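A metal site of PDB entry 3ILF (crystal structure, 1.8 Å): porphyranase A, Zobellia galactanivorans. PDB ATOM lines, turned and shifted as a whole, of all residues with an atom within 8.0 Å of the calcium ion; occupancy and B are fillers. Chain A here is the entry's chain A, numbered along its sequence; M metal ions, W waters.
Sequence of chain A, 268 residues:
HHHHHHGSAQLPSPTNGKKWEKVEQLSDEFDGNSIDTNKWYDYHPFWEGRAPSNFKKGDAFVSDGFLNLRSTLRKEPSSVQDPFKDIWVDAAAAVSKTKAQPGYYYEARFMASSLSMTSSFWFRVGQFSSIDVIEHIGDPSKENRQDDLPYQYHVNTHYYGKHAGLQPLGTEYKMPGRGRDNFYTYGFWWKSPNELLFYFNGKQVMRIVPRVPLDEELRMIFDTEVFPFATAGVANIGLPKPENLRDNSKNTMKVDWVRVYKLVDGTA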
ATOM      1  N   ASP A  28     -24.567 -26.306 -19.798  1.00  0.00           N
ATOM      2  CA  ASP A  28     -24.569 -25.485 -20.994  1.00  0.00           C
ATOM      3  C   ASP A  28     -26.017 -25.281 -21.415  1.00  0.00           C
ATOM      4  O   ASP A  28     -26.788 -26.240 -21.462  1.00  0.00           O
ATOM      5  CB  ASP A  28     -23.761 -26.188 -22.121  1.00  0.00           C
ATOM      6  CG  ASP A  28     -23.172 -25.228 -23.182  1.00  0.00           C
ATOM      7  OD1 ASP A  28     -23.824 -24.215 -23.484  1.00  0.00           O
ATOM      8  OD2 ASP A  28     -22.073 -25.501 -23.691  1.00  0.00           O
ATOM      9  N   GLU A  29     -26.338 -24.040 -21.777  1.00  0.00           N
ATOM     10  CA  GLU A  29     -27.655 -23.668 -22.292  1.00  0.00           C
ATOM     11  C   GLU A  29     -27.709 -23.832 -23.818  1.00  0.00           C
ATOM     12  O   GLU A  29     -28.809 -23.753 -24.456  1.00  0.00           O
ATOM     13  CB  GLU A  29     -27.952 -22.202 -21.910  1.00  0.00           C
ATOM     14  CG  GLU A  29     -28.115 -22.026 -20.393  1.00  0.00           C
ATOM     15  CD  GLU A  29     -29.211 -22.909 -19.807  1.00  0.00           C
ATOM     16  OE1 GLU A  29     -30.386 -22.913 -20.302  1.00  0.00           O
ATOM     17  OE2 GLU A  29     -28.895 -23.595 -18.794  1.00  0.00           O
ATOM     18  N   PHE A  30     -26.537 -23.991 -24.410  1.00  0.00           N
ATOM     19  CA  PHE A  30     -26.403 -24.251 -25.853  1.00  0.00           C
ATOM     20  C   PHE A  30     -27.037 -23.133 -26.684  1.00  0.00           C
ATOM     21  O   PHE A  30     -27.636 -23.366 -27.744  1.00  0.00           O
ATOM     22  CB  PHE A  30     -27.023 -25.614 -26.197  1.00  0.00           C
ATOM     23  CG  PHE A  30     -26.306 -26.762 -25.564  1.00  0.00           C
ATOM     24  CD1 PHE A  30     -24.927 -26.949 -25.765  1.00  0.00           C
ATOM     25  CD2 PHE A  30     -27.025 -27.702 -24.801  1.00  0.00           C
ATOM     26  CE1 PHE A  30     -24.267 -28.032 -25.188  1.00  0.00           C
ATOM     27  CE2 PHE A  30     -26.346 -28.802 -24.184  1.00  0.00           C
ATOM     28  CZ  PHE A  30     -24.978 -28.964 -24.375  1.00  0.00           C
ATOM     29  N   ASP A  31     -26.914 -21.915 -26.174  1.00  0.00           N
ATOM     30  CA  ASP A  31     -27.608 -20.796 -26.773  1.00  0.00           C
ATOM     31  C   ASP A  31     -26.668 -19.964 -27.627  1.00  0.00           C
ATOM     32  O   ASP A  31     -27.041 -18.896 -28.118  1.00  0.00           O
ATOM     33  CB  ASP A  31     -28.263 -19.916 -25.682  1.00  0.00           C
ATOM     34  CG  ASP A  31     -29.495 -20.578 -25.093  1.00  0.00           C
ATOM     35  OD1 ASP A  31     -29.979 -21.569 -25.738  1.00  0.00           O
ATOM     36  OD2 ASP A  31     -30.061 -20.096 -24.041  1.00  0.00           O
ATOM     37  N   GLY A  32     -25.465 -20.465 -27.883  1.00  0.00           N
ATOM     38  CA  GLY A  32     -24.598 -19.699 -28.768  1.00  0.00           C
ATOM     39  C   GLY A  32     -24.644 -20.065 -30.237  1.00  0.00           C
ATOM     40  O   GLY A  32     -25.531 -20.794 -30.754  1.00  0.00           O
ATOM     41  N   VAL A  62     -24.303 -27.044 -32.258  1.00  0.00           N
ATOM     42  CA  VAL A  62     -25.131 -26.071 -31.521  1.00  0.00           C
ATOM     43  C   VAL A  62     -25.756 -25.047 -32.474  1.00  0.00           C
ATOM     44  O   VAL A  62     -25.013 -24.407 -33.301  1.00  0.00           O
ATOM     45  CB  VAL A  62     -24.266 -25.425 -30.437  1.00  0.00           C
ATOM     46  CG1 VAL A  62     -25.054 -24.199 -29.776  1.00  0.00           C
ATOM     47  CG2 VAL A  62     -23.921 -26.527 -29.363  1.00  0.00           C
ATOM     48  N   SER A  63     -27.080 -24.899 -32.400  1.00  0.00           N
ATOM     49  CA  SER A  63     -27.805 -23.954 -33.263  1.00  0.00           C
ATOM     50  C   SER A  63     -29.215 -23.775 -32.740  1.00  0.00           C
ATOM     51  O   SER A  63     -29.788 -24.714 -32.225  1.00  0.00           O
ATOM     52  CB  SER A  63     -27.928 -24.559 -34.667  1.00  0.00           C
ATOM     53  OG  SER A  63     -28.472 -23.523 -35.488  1.00  0.00           O
ATOM     54  N   ASP A  64     -29.788 -22.549 -32.845  1.00  0.00           N
ATOM     55  CA  ASP A  64     -31.252 -22.356 -32.528  1.00  0.00           C
ATOM     56  C   ASP A  64     -31.606 -22.610 -31.057  1.00  0.00           C
ATOM     57  O   ASP A  64     -32.764 -22.823 -30.741  1.00  0.00           O
ATOM     58  CB  ASP A  64     -32.124 -23.263 -33.391  1.00  0.00           C
ATOM     59  CG  ASP A  64     -32.570 -22.633 -34.713  1.00  0.00           C
ATOM     60  OD1 ASP A  64     -32.012 -21.587 -35.087  1.00  0.00           O
ATOM     61  OD2 ASP A  64     -33.499 -23.258 -35.382  1.00  0.00           O
ATOM     62  N   GLY A  65     -30.576 -22.598 -30.215  1.00  0.00           N
ATOM     63  CA  GLY A  65     -30.751 -22.741 -28.754  1.00  0.00           C
ATOM     64  C   GLY A  65     -30.566 -24.169 -28.275  1.00  0.00           C
ATOM     65  O   GLY A  65     -30.837 -24.449 -27.130  1.00  0.00           O
ATOM     66  N   PHE A  66     -30.075 -25.063 -29.125  1.00  0.00           N
ATOM     67  CA  PHE A  66     -30.099 -26.513 -28.765  1.00  0.00           C
ATOM     68  C   PHE A  66     -28.726 -27.014 -29.122  1.00  0.00           C
ATOM     69  O   PHE A  66     -28.048 -26.485 -30.124  1.00  0.00           O
ATOM     70  CB  PHE A  66     -31.061 -27.290 -29.673  1.00  0.00           C
ATOM     71  CG  PHE A  66     -32.453 -26.858 -29.543  1.00  0.00           C
ATOM     72  CD1 PHE A  66     -33.161 -27.125 -28.373  1.00  0.00           C
ATOM     73  CD2 PHE A  66     -33.097 -26.208 -30.659  1.00  0.00           C
ATOM     74  CE1 PHE A  66     -34.538 -26.727 -28.244  1.00  0.00           C
ATOM     75  CE2 PHE A  66     -34.416 -25.756 -30.541  1.00  0.00           C
ATOM     76  CZ  PHE A  66     -35.141 -26.026 -29.343  1.00  0.00           C
ATOM     77  N   LEU A  67     -28.330 -28.082 -28.394  1.00  0.00           N
ATOM     78  CA  LEU A  67     -27.310 -28.965 -28.937  1.00  0.00           C
ATOM     79  C   LEU A  67     -28.105 -29.954 -29.782  1.00  0.00           C
ATOM     80  O   LEU A  67     -28.970 -30.702 -29.228  1.00  0.00           O
ATOM     81  CB  LEU A  67     -26.602 -29.757 -27.810  1.00  0.00           C
ATOM     82  CG  LEU A  67     -25.665 -30.863 -28.335  1.00  0.00           C
ATOM     83  CD1 LEU A  67     -24.428 -30.372 -29.178  1.00  0.00           C
ATOM     84  CD2 LEU A  67     -25.153 -31.784 -27.153  1.00  0.00           C
ATOM     85  N   ARG A 109     -32.717 -31.314 -20.587  1.00  0.00           N
ATOM     86  CA  ARG A 109     -34.027 -31.181 -21.190  1.00  0.00           C
ATOM     87  C   ARG A 109     -33.877 -31.372 -22.684  1.00  0.00           C
ATOM     88  O   ARG A 109     -33.140 -30.628 -23.354  1.00  0.00           O
ATOM     89  CB  ARG A 109     -34.663 -29.846 -20.834  1.00  0.00           C
ATOM     90  CG  ARG A 109     -36.109 -29.786 -21.164  1.00  0.00           C
ATOM     91  CD  ARG A 109     -36.686 -28.444 -20.705  1.00  0.00           C
ATOM     92  NE  ARG A 109     -38.032 -28.274 -21.236  1.00  0.00           N
ATOM     93  CZ  ARG A 109     -39.101 -28.919 -20.782  1.00  0.00           C
ATOM     94  NH1 ARG A 109     -39.008 -29.790 -19.766  1.00  0.00           N
ATOM     95  NH2 ARG A 109     -40.283 -28.658 -21.387  1.00  0.00           N
ATOM     96  N   VAL A 255     -31.223 -31.006 -27.607  1.00  0.00           N
ATOM     97  CA  VAL A 255     -31.037 -30.825 -26.167  1.00  0.00           C
ATOM     98  C   VAL A 255     -31.059 -29.340 -25.948  1.00  0.00           C
ATOM     99  O   VAL A 255     -30.155 -28.629 -26.452  1.00  0.00           O
ATOM    100  CB  VAL A 255     -29.672 -31.420 -25.718  1.00  0.00           C
ATOM    101  CG1 VAL A 255     -29.491 -31.245 -24.191  1.00  0.00           C
ATOM    102  CG2 VAL A 255     -29.636 -32.935 -26.067  1.00  0.00           C
ATOM    103  N   ASP A 256     -32.061 -28.854 -25.205  1.00  0.00           N
ATOM    104  CA  ASP A 256     -32.181 -27.373 -24.978  1.00  0.00           C
ATOM    105  C   ASP A 256     -31.088 -26.975 -23.993  1.00  0.00           C
ATOM    106  O   ASP A 256     -30.505 -25.888 -24.049  1.00  0.00           O
ATOM    107  CB  ASP A 256     -33.564 -27.113 -24.308  1.00  0.00           C
ATOM    108  CG  ASP A 256     -33.911 -25.623 -24.191  1.00  0.00           C
ATOM    109  OD1 ASP A 256     -33.179 -24.751 -24.700  1.00  0.00           O
ATOM    110  OD2 ASP A 256     -34.999 -25.396 -23.560  1.00  0.00           O
ATOM    111  N   TRP A 257     -30.803 -27.855 -23.019  1.00  0.00           N
ATOM    112  CA  TRP A 257     -29.768 -27.541 -22.069  1.00  0.00           C
ATOM    113  C   TRP A 257     -29.430 -28.713 -21.230  1.00  0.00           C
ATOM    114  O   TRP A 257     -30.217 -29.683 -21.147  1.00  0.00           O
ATOM    115  CB  TRP A 257     -30.241 -26.404 -21.117  1.00  0.00           C
ATOM    116  CG  TRP A 257     -31.646 -26.497 -20.492  1.00  0.00           C
ATOM    117  CD1 TRP A 257     -32.720 -25.732 -20.837  1.00  0.00           C
ATOM    118  CD2 TRP A 257     -32.086 -27.320 -19.375  1.00  0.00           C
ATOM    119  NE1 TRP A 257     -33.819 -26.027 -20.012  1.00  0.00           N
ATOM    120  CE2 TRP A 257     -33.444 -26.988 -19.107  1.00  0.00           C
ATOM    121  CE3 TRP A 257     -31.436 -28.323 -18.566  1.00  0.00           C
ATOM    122  CZ2 TRP A 257     -34.195 -27.585 -18.058  1.00  0.00           C
ATOM    123  CZ3 TRP A 257     -32.221 -28.976 -17.533  1.00  0.00           C
ATOM    124  CH2 TRP A 257     -33.571 -28.585 -17.301  1.00  0.00           C
ATOM    125  N   VAL A 258     -28.217 -28.669 -20.673  1.00  0.00           N
ATOM    126  CA  VAL A 258     -27.773 -29.604 -19.645  1.00  0.00           C
ATOM    127  C   VAL A 258     -27.277 -28.809 -18.421  1.00  0.00           C
ATOM    128  O   VAL A 258     -26.612 -27.782 -18.563  1.00  0.00           O
ATOM    129  CB  VAL A 258     -26.713 -30.643 -20.228  1.00  0.00           C
ATOM    130  CG1 VAL A 258     -25.407 -29.954 -20.651  1.00  0.00           C
ATOM    131  CG2 VAL A 258     -26.410 -31.753 -19.156  1.00  0.00           C
ATOM    132  N   ARG A 259     -27.669 -29.251 -17.226  1.00  0.00           N
ATOM    133  CA  ARG A 259     -27.246 -28.520 -16.019  1.00  0.00           C
ATOM    134  C   ARG A 259     -26.803 -29.541 -15.021  1.00  0.00           C
ATOM    135  O   ARG A 259     -27.488 -30.536 -14.778  1.00  0.00           O
ATOM    136  CB  ARG A 259     -28.409 -27.668 -15.445  1.00  0.00           C
ATOM    137  CG  ARG A 259     -28.875 -26.532 -16.446  1.00  0.00           C
ATOM    138  CD  ARG A 259     -30.238 -25.934 -15.994  1.00  0.00           C
ATOM    139  NE  ARG A 259     -30.698 -24.961 -16.993  1.00  0.00           N
ATOM    140  CZ  ARG A 259     -31.940 -24.463 -17.026  1.00  0.00           C
ATOM    141  NH1 ARG A 259     -32.872 -24.846 -16.099  1.00  0.00           N
ATOM    142  NH2 ARG A 259     -32.249 -23.585 -18.002  1.00  0.00           N
HETATM  143 CA    CA M   1     -31.059 -23.722 -24.929  1.00  0.00          CA
HETATM  144  O   HOH W   1     -31.488 -22.816 -22.674  1.00  0.00           O
HETATM  145  O   HOH W   2     -32.790 -22.179 -25.573  1.00  0.00           O
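The calcium ion is bound by O of Glu 29 (2.3 Å). The calcium ion is bound by O of Gly 65. OD1 of Asp 256 binds the calcium ion (2.4 Å). The calcium ion is bound by O of Asp 256 (2.4 Å). Water W2 binds the calcium ion, 2.4 Å away. Water W1 binds the calcium ion (2.5 Å). The side-chain carboxylate (OD1) of Asp 31 binds the calcium ion, 2.5 Å away. The calcium ion has seven donor atoms within binding distance.
The side-chain carboxylate (OE2) of Glu 29 is in salt-bridge range of the guanidinium group (NE) of Arg 259 (2.9 Å). The backbone carbonyl oxygen (O) of Arg 109 lies within hydrogen-bond range of the backbone NH (N) of Asp 256 (2.8 Å).
Four residues have an atom within 4 Å of the calcium ion: Glu 29, Asp 31, Gly 65 and Asp 256.
Water W1 lies within hydrogen-bond range of the side-chain carboxylate of Glu 29 (2.6 Å) and the side-chain carboxylate of Asp 31 (3.4 Å).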
